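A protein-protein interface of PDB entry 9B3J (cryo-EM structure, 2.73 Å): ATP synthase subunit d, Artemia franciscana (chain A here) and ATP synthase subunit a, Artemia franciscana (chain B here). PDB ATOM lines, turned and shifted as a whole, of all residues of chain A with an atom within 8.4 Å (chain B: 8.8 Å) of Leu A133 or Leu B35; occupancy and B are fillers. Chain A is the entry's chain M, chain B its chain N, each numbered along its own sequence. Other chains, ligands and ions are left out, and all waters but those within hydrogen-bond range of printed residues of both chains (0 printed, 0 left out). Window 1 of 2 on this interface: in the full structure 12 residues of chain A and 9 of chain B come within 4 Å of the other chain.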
ATOM      1  N   ILE A 126      22.619 -21.456  23.391  1.00  0.00           N
ATOM      2  CA  ILE A 126      23.567 -22.413  23.972  1.00  0.00           C
ATOM      3  C   ILE A 126      24.842 -22.415  23.137  1.00  0.00           C
ATOM      4  O   ILE A 126      24.760 -22.340  21.897  1.00  0.00           O
ATOM      5  CB  ILE A 126      22.927 -23.804  24.037  1.00  0.00           C
ATOM      6  CG1 ILE A 126      23.957 -24.894  24.307  1.00  0.00           C
ATOM      7  CG2 ILE A 126      22.155 -24.099  22.769  1.00  0.00           C
ATOM      8  CD1 ILE A 126      23.357 -26.259  24.443  1.00  0.00           C
ATOM      9  N   PRO A 127      26.027 -22.430  23.752  1.00  0.00           N
ATOM     10  CA  PRO A 127      27.271 -22.391  22.973  1.00  0.00           C
ATOM     11  C   PRO A 127      27.439 -23.627  22.107  1.00  0.00           C
ATOM     12  O   PRO A 127      26.964 -24.712  22.442  1.00  0.00           O
ATOM     13  CB  PRO A 127      28.359 -22.320  24.048  1.00  0.00           C
ATOM     14  CG  PRO A 127      27.670 -21.774  25.245  1.00  0.00           C
ATOM     15  CD  PRO A 127      26.278 -22.298  25.196  1.00  0.00           C
ATOM     16  N   PHE A 128      28.134 -23.451  20.981  1.00  0.00           N
ATOM     17  CA  PHE A 128      28.276 -24.531  20.010  1.00  0.00           C
ATOM     18  C   PHE A 128      29.100 -25.700  20.533  1.00  0.00           C
ATOM     19  O   PHE A 128      29.038 -26.789  19.955  1.00  0.00           O
ATOM     20  CB  PHE A 128      28.915 -24.013  18.725  1.00  0.00           C
ATOM     21  CG  PHE A 128      28.160 -22.896  18.080  1.00  0.00           C
ATOM     22  CD1 PHE A 128      26.921 -23.117  17.515  1.00  0.00           C
ATOM     23  CD2 PHE A 128      28.698 -21.627  18.024  1.00  0.00           C
ATOM     24  CE1 PHE A 128      26.229 -22.089  16.914  1.00  0.00           C
ATOM     25  CE2 PHE A 128      28.011 -20.597  17.424  1.00  0.00           C
ATOM     26  CZ  PHE A 128      26.774 -20.830  16.869  1.00  0.00           C
ATOM     27  N   GLU A 129      29.875 -25.505  21.596  1.00  0.00           N
ATOM     28  CA  GLU A 129      30.649 -26.611  22.141  1.00  0.00           C
ATOM     29  C   GLU A 129      29.756 -27.617  22.853  1.00  0.00           C
ATOM     30  O   GLU A 129      30.027 -28.822  22.812  1.00  0.00           O
ATOM     31  CB  GLU A 129      31.727 -26.083  23.086  1.00  0.00           C
ATOM     32  CG  GLU A 129      32.841 -25.302  22.397  1.00  0.00           C
ATOM     33  CD  GLU A 129      32.469 -23.857  22.101  1.00  0.00           C
ATOM     34  OE1 GLU A 129      31.591 -23.311  22.801  1.00  0.00           O
ATOM     35  OE2 GLU A 129      33.050 -23.270  21.167  1.00  0.00           O
ATOM     36  N   HIS A 130      28.693 -27.146  23.498  1.00  0.00           N
ATOM     37  CA  HIS A 130      27.758 -28.001  24.210  1.00  0.00           C
ATOM     38  C   HIS A 130      26.481 -28.249  23.420  1.00  0.00           C
ATOM     39  O   HIS A 130      25.497 -28.733  23.987  1.00  0.00           O
ATOM     40  CB  HIS A 130      27.413 -27.385  25.564  1.00  0.00           C
ATOM     41  CG  HIS A 130      28.580 -26.756  26.256  1.00  0.00           C
ATOM     42  ND1 HIS A 130      29.829 -27.336  26.287  1.00  0.00           N
ATOM     43  CD2 HIS A 130      28.687 -25.594  26.943  1.00  0.00           C
ATOM     44  CE1 HIS A 130      30.655 -26.558  26.964  1.00  0.00           C
ATOM     45  NE2 HIS A 130      29.986 -25.496  27.373  1.00  0.00           N
ATOM     46  N   MET A 131      26.474 -27.923  22.133  1.00  0.00           N
ATOM     47  CA  MET A 131      25.268 -27.970  21.320  1.00  0.00           C
ATOM     48  C   MET A 131      25.138 -29.337  20.663  1.00  0.00           C
ATOM     49  O   MET A 131      26.027 -29.755  19.916  1.00  0.00           O
ATOM     50  CB  MET A 131      25.303 -26.877  20.257  1.00  0.00           C
ATOM     51  CG  MET A 131      24.033 -26.053  20.161  1.00  0.00           C
ATOM     52  SD  MET A 131      24.076 -24.892  18.788  1.00  0.00           S
ATOM     53  CE  MET A 131      22.597 -23.942  19.105  1.00  0.00           C
ATOM     54  N   THR A 132      24.036 -30.029  20.945  1.00  0.00           N
ATOM     55  CA  THR A 132      23.693 -31.233  20.207  1.00  0.00           C
ATOM     56  C   THR A 132      23.194 -30.854  18.818  1.00  0.00           C
ATOM     57  O   THR A 132      22.845 -29.703  18.553  1.00  0.00           O
ATOM     58  CB  THR A 132      22.617 -32.026  20.933  1.00  0.00           C
ATOM     59  OG1 THR A 132      21.339 -31.479  20.601  1.00  0.00           O
ATOM     60  CG2 THR A 132      22.803 -31.929  22.426  1.00  0.00           C
ATOM     61  N   LEU A 133      23.136 -31.838  17.923  1.00  0.00           N
ATOM     62  CA  LEU A 133      22.768 -31.519  16.550  1.00  0.00           C
ATOM     63  C   LEU A 133      21.292 -31.204  16.383  1.00  0.00           C
ATOM     64  O   LEU A 133      20.890 -30.797  15.292  1.00  0.00           O
ATOM     65  CB  LEU A 133      23.158 -32.655  15.617  1.00  0.00           C
ATOM     66  CG  LEU A 133      24.324 -32.260  14.719  1.00  0.00           C
ATOM     67  CD1 LEU A 133      24.873 -33.439  13.965  1.00  0.00           C
ATOM     68  CD2 LEU A 133      23.851 -31.218  13.756  1.00  0.00           C
ATOM     69  N   GLU A 134      20.476 -31.395  17.417  1.00  0.00           N
ATOM     70  CA  GLU A 134      19.080 -30.985  17.366  1.00  0.00           C
ATOM     71  C   GLU A 134      18.838 -29.614  17.970  1.00  0.00           C
ATOM     72  O   GLU A 134      17.958 -28.891  17.492  1.00  0.00           O
ATOM     73  CB  GLU A 134      18.191 -32.006  18.078  1.00  0.00           C
ATOM     74  CG  GLU A 134      17.911 -33.236  17.248  1.00  0.00           C
ATOM     75  CD  GLU A 134      16.709 -34.000  17.742  1.00  0.00           C
ATOM     76  OE1 GLU A 134      16.213 -33.678  18.841  1.00  0.00           O
ATOM     77  OE2 GLU A 134      16.250 -34.915  17.028  1.00  0.00           O
ATOM     78  N   ASP A 135      19.589 -29.236  19.006  1.00  0.00           N
ATOM     79  CA  ASP A 135      19.498 -27.872  19.516  1.00  0.00           C
ATOM     80  C   ASP A 135      19.984 -26.862  18.492  1.00  0.00           C
ATOM     81  O   ASP A 135      19.457 -25.744  18.423  1.00  0.00           O
ATOM     82  CB  ASP A 135      20.295 -27.739  20.806  1.00  0.00           C
ATOM     83  CG  ASP A 135      19.642 -28.450  21.955  1.00  0.00           C
ATOM     84  OD1 ASP A 135      18.565 -29.043  21.742  1.00  0.00           O
ATOM     85  OD2 ASP A 135      20.201 -28.418  23.070  1.00  0.00           O
ATOM     86  N   PHE A 136      20.985 -27.235  17.697  1.00  0.00           N
ATOM     87  CA  PHE A 136      21.397 -26.388  16.588  1.00  0.00           C
ATOM     88  C   PHE A 136      20.286 -26.260  15.562  1.00  0.00           C
ATOM     89  O   PHE A 136      20.053 -25.174  15.022  1.00  0.00           O
ATOM     90  CB  PHE A 136      22.659 -26.946  15.943  1.00  0.00           C
ATOM     91  CG  PHE A 136      23.081 -26.210  14.721  1.00  0.00           C
ATOM     92  CD1 PHE A 136      23.691 -24.979  14.820  1.00  0.00           C
ATOM     93  CD2 PHE A 136      22.878 -26.751  13.472  1.00  0.00           C
ATOM     94  CE1 PHE A 136      24.088 -24.302  13.696  1.00  0.00           C
ATOM     95  CE2 PHE A 136      23.267 -26.078  12.351  1.00  0.00           C
ATOM     96  CZ  PHE A 136      23.875 -24.852  12.461  1.00  0.00           C
ATOM     97  N   PHE A 137      19.586 -27.352  15.281  1.00  0.00           N
ATOM     98  CA  PHE A 137      18.495 -27.278  14.325  1.00  0.00           C
ATOM     99  C   PHE A 137      17.260 -26.611  14.904  1.00  0.00           C
ATOM    100  O   PHE A 137      16.421 -26.131  14.137  1.00  0.00           O
ATOM    101  CB  PHE A 137      18.155 -28.670  13.807  1.00  0.00           C
ATOM    102  CG  PHE A 137      19.136 -29.190  12.803  1.00  0.00           C
ATOM    103  CD1 PHE A 137      20.024 -28.337  12.175  1.00  0.00           C
ATOM    104  CD2 PHE A 137      19.166 -30.529  12.480  1.00  0.00           C
ATOM    105  CE1 PHE A 137      20.926 -28.813  11.251  1.00  0.00           C
ATOM    106  CE2 PHE A 137      20.064 -31.008  11.556  1.00  0.00           C
ATOM    107  CZ  PHE A 137      20.945 -30.149  10.943  1.00  0.00           C
ATOM    108  N   GLU A 138      17.127 -26.558  16.229  1.00  0.00           N
ATOM    109  CA  GLU A 138      16.053 -25.760  16.807  1.00  0.00           C
ATOM    110  C   GLU A 138      16.366 -24.274  16.720  1.00  0.00           C
ATOM    111  O   GLU A 138      15.490 -23.467  16.388  1.00  0.00           O
ATOM    112  CB  GLU A 138      15.805 -26.169  18.253  1.00  0.00           C
ATOM    113  CG  GLU A 138      15.068 -27.478  18.391  1.00  0.00           C
ATOM    114  CD  GLU A 138      14.556 -27.702  19.792  1.00  0.00           C
ATOM    115  OE1 GLU A 138      14.607 -26.748  20.597  1.00  0.00           O
ATOM    116  OE2 GLU A 138      14.103 -28.827  20.091  1.00  0.00           O
ATOM    117  N   ALA A 139      17.611 -23.893  17.010  1.00  0.00           N
ATOM    118  CA  ALA A 139      17.992 -22.490  16.936  1.00  0.00           C
ATOM    119  C   ALA A 139      18.183 -22.004  15.507  1.00  0.00           C
ATOM    120  O   ALA A 139      18.206 -20.792  15.280  1.00  0.00           O
ATOM    121  CB  ALA A 139      19.274 -22.248  17.729  1.00  0.00           C
ATOM    122  N   PHE A 140      18.333 -22.912  14.548  1.00  0.00           N
ATOM    123  CA  PHE A 140      18.479 -22.560  13.138  1.00  0.00           C
ATOM    124  C   PHE A 140      17.498 -23.414  12.353  1.00  0.00           C
ATOM    125  O   PHE A 140      17.838 -24.509  11.889  1.00  0.00           O
ATOM    126  CB  PHE A 140      19.910 -22.760  12.662  1.00  0.00           C
ATOM    127  CG  PHE A 140      20.890 -21.849  13.326  1.00  0.00           C
ATOM    128  CD1 PHE A 140      21.447 -22.179  14.546  1.00  0.00           C
ATOM    129  CD2 PHE A 140      21.255 -20.660  12.729  1.00  0.00           C
ATOM    130  CE1 PHE A 140      22.347 -21.341  15.158  1.00  0.00           C
ATOM    131  CE2 PHE A 140      22.155 -19.819  13.336  1.00  0.00           C
ATOM    132  CZ  PHE A 140      22.702 -20.159  14.552  1.00  0.00           C
ATOM    133  N   LYS A 143      17.101 -26.449   8.788  1.00  0.00           N
ATOM    134  CA  LYS A 143      17.110 -27.912   8.964  1.00  0.00           C
ATOM    135  C   LYS A 143      17.371 -28.601   7.624  1.00  0.00           C
ATOM    136  O   LYS A 143      18.016 -28.037   6.730  1.00  0.00           O
ATOM    137  CB  LYS A 143      15.826 -28.359   9.636  1.00  0.00           C
ATOM    138  CG  LYS A 143      15.726 -28.048  11.111  1.00  0.00           C
ATOM    139  CD  LYS A 143      14.462 -28.666  11.691  1.00  0.00           C
ATOM    140  CE  LYS A 143      14.372 -28.489  13.198  1.00  0.00           C
ATOM    141  NZ  LYS A 143      14.257 -27.059  13.596  1.00  0.00           N
ATOM    142  N   MET B  31      27.900 -42.571  13.854  1.00  0.00           N
ATOM    143  CA  MET B  31      26.671 -41.927  14.277  1.00  0.00           C
ATOM    144  C   MET B  31      26.992 -40.540  14.807  1.00  0.00           C
ATOM    145  O   MET B  31      27.953 -40.361  15.558  1.00  0.00           O
ATOM    146  CB  MET B  31      25.959 -42.751  15.346  1.00  0.00           C
ATOM    147  CG  MET B  31      25.067 -43.844  14.793  1.00  0.00           C
ATOM    148  SD  MET B  31      24.252 -44.741  16.123  1.00  0.00           S
ATOM    149  CE  MET B  31      23.114 -45.762  15.204  1.00  0.00           C
ATOM    150  N   SER B  32      26.178 -39.565  14.414  1.00  0.00           N
ATOM    151  CA  SER B  32      26.429 -38.158  14.689  1.00  0.00           C
ATOM    152  C   SER B  32      25.449 -37.657  15.739  1.00  0.00           C
ATOM    153  O   SER B  32      24.237 -37.720  15.539  1.00  0.00           O
ATOM    154  CB  SER B  32      26.316 -37.336  13.410  1.00  0.00           C
ATOM    155  OG  SER B  32      25.125 -37.648  12.717  1.00  0.00           O
ATOM    156  N   PHE B  33      25.979 -37.160  16.849  1.00  0.00           N
ATOM    157  CA  PHE B  33      25.176 -36.589  17.919  1.00  0.00           C
ATOM    158  C   PHE B  33      25.496 -35.126  18.167  1.00  0.00           C
ATOM    159  O   PHE B  33      24.588 -34.291  18.157  1.00  0.00           O
ATOM    160  CB  PHE B  33      25.382 -37.394  19.204  1.00  0.00           C
ATOM    161  CG  PHE B  33      24.596 -36.899  20.371  1.00  0.00           C
ATOM    162  CD1 PHE B  33      23.299 -37.282  20.548  1.00  0.00           C
ATOM    163  CD2 PHE B  33      25.174 -36.095  21.318  1.00  0.00           C
ATOM    164  CE1 PHE B  33      22.582 -36.845  21.628  1.00  0.00           C
ATOM    165  CE2 PHE B  33      24.457 -35.655  22.396  1.00  0.00           C
ATOM    166  CZ  PHE B  33      23.163 -36.034  22.550  1.00  0.00           C
ATOM    167  N   TRP B  34      26.760 -34.785  18.392  1.00  0.00           N
ATOM    168  CA  TRP B  34      27.090 -33.410  18.722  1.00  0.00           C
ATOM    169  C   TRP B  34      27.256 -32.578  17.459  1.00  0.00           C
ATOM    170  O   TRP B  34      27.446 -33.101  16.360  1.00  0.00           O
ATOM    171  CB  TRP B  34      28.365 -33.337  19.549  1.00  0.00           C
ATOM    172  CG  TRP B  34      28.291 -34.021  20.860  1.00  0.00           C
ATOM    173  CD1 TRP B  34      28.826 -35.223  21.176  1.00  0.00           C
ATOM    174  CD2 TRP B  34      27.652 -33.541  22.044  1.00  0.00           C
ATOM    175  NE1 TRP B  34      28.563 -35.527  22.484  1.00  0.00           N
ATOM    176  CE2 TRP B  34      27.842 -34.506  23.038  1.00  0.00           C
ATOM    177  CE3 TRP B  34      26.942 -32.388  22.359  1.00  0.00           C
ATOM    178  CZ2 TRP B  34      27.348 -34.357  24.320  1.00  0.00           C
ATOM    179  CZ3 TRP B  34      26.456 -32.243  23.633  1.00  0.00           C
ATOM    180  CH2 TRP B  34      26.658 -33.221  24.596  1.00  0.00           C
ATOM    181  N   LEU B  35      27.181 -31.258  17.632  1.00  0.00           N
ATOM    182  CA  LEU B  35      27.249 -30.359  16.486  1.00  0.00           C
ATOM    183  C   LEU B  35      28.648 -30.329  15.895  1.00  0.00           C
ATOM    184  O   LEU B  35      28.819 -30.424  14.675  1.00  0.00           O
ATOM    185  CB  LEU B  35      26.809 -28.958  16.892  1.00  0.00           C
ATOM    186  CG  LEU B  35      26.928 -27.893  15.812  1.00  0.00           C
ATOM    187  CD1 LEU B  35      26.041 -28.222  14.636  1.00  0.00           C
ATOM    188  CD2 LEU B  35      26.557 -26.559  16.398  1.00  0.00           C
ATOM    189  N   ILE B  36      29.661 -30.190  16.741  1.00  0.00           N
ATOM    190  CA  ILE B  36      31.050 -30.282  16.307  1.00  0.00           C
ATOM    191  C   ILE B  36      31.421 -31.756  16.309  1.00  0.00           C
ATOM    192  O   ILE B  36      31.306 -32.418  17.346  1.00  0.00           O
ATOM    193  CB  ILE B  36      31.978 -29.460  17.208  1.00  0.00           C
ATOM    194  CG1 ILE B  36      31.443 -29.448  18.638  1.00  0.00           C
ATOM    195  CG2 ILE B  36      32.109 -28.049  16.680  1.00  0.00           C
ATOM    196  CD1 ILE B  36      32.371 -28.796  19.616  1.00  0.00           C
ATOM    197  N   PRO B  37      31.852 -32.310  15.185  1.00  0.00           N
ATOM    198  CA  PRO B  37      31.984 -33.765  15.080  1.00  0.00           C
ATOM    199  C   PRO B  37      33.164 -34.288  15.883  1.00  0.00           C
ATOM    200  O   PRO B  37      34.026 -33.543  16.341  1.00  0.00           O
ATOM    201  CB  PRO B  37      32.178 -33.997  13.581  1.00  0.00           C
ATOM    202  CG  PRO B  37      32.639 -32.711  13.039  1.00  0.00           C
ATOM    203  CD  PRO B  37      32.133 -31.624  13.917  1.00  0.00           C
ATOM    204  N   SER B  38      33.171 -35.601  16.080  1.00  0.00           N
ATOM    205  CA  SER B  38      34.310 -36.251  16.702  1.00  0.00           C
ATOM    206  C   SER B  38      35.376 -36.523  15.652  1.00  0.00           C
ATOM    207  O   SER B  38      35.236 -36.165  14.482  1.00  0.00           O
ATOM    208  CB  SER B  38      33.877 -37.539  17.388  1.00  0.00           C
ATOM    209  OG  SER B  38      33.274 -38.414  16.456  1.00  0.00           O
ATOM    210  N   GLN B  41      33.955 -39.331  12.969  1.00  0.00           N
ATOM    211  CA  GLN B  41      32.915 -38.757  12.129  1.00  0.00           C
ATOM    212  C   GLN B  41      33.496 -37.752  11.151  1.00  0.00           C
ATOM    213  O   GLN B  41      33.129 -37.741   9.972  1.00  0.00           O
ATOM    214  CB  GLN B  41      31.851 -38.095  12.993  1.00  0.00           C
ATOM    215  CG  GLN B  41      30.767 -37.425  12.194  1.00  0.00           C
ATOM    216  CD  GLN B  41      29.851 -36.599  13.054  1.00  0.00           C
ATOM    217  OE1 GLN B  41      29.822 -36.743  14.277  1.00  0.00           O
ATOM    218  NE2 GLN B  41      29.106 -35.708  12.421  1.00  0.00           N
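The backbone NH (N) of Leu A133 is in hydrogen-bond range of the backbone carbonyl oxygen (O) of Phe B33, at 2.9 Å.
The backbone carbonyl oxygen (O) of Met A131 sits at hydrogen-bond distance from the backbone NH (N) of Leu B35.
The backbone NH of Glu A134 lies close to the side-chain hydroxyl of Thr A132 (3.3 Å).
The side-chain hydroxyl (OG1) of Thr A132 lies within hydrogen-bond range of the backbone NH (N) of Asp A135.
Phe A128 touches Leu B35 (CD1 to CD2, 3.6 Å).
Ile B36 touches Phe A128 (CG1 to O, 3.8 Å).
Glu A129 touches Ile B36.
His A130 touches Trp B34 (O to CZ3, 3.7 Å).
Met A131 touches Trp B34 (O to CE3, 3.7 Å).
Thr A132 touches Phe B33.
Thr A132 touches Trp B34.
Leu A133 touches Trp B34 (CD1 to O, 3.5 Å).
CD2 of Leu A133 touches CD1 of Leu B35 (3.8 Å).
Leu B35 touches Phe A136 (CD1 to CG, 3.6 Å).
Leu A133 touches just these residues of chain B: Phe B33 (2.9 Å), Trp B34 (3.5 Å) and Leu B35 (3.8 Å).
Leu B35 touches just these residues of chain A: Phe A128, Met A131, Leu A133 and Phe A136.
Thr A132 touches two residues of chain B.
Of the printed residues of chain B, Met A131 touches Trp B34 and Leu B35.
Printed residues of chain A within 4 Å of Phe B33: Thr A132 and Leu A133.
Phe A140 touches none of the printed residues of chain B.
Of the 9 printed residues of chain B, 4 touch a printed residue of chain A.
Printed residues of chain B that touch a printed residue of chain A: Phe B33, Trp B34, Leu B35 and Ile B36.
Hydrophobic or aromatic side chains of chain B within 4 Å of the printed part of chain A: Trp B34, Leu B35 and Ile B36.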
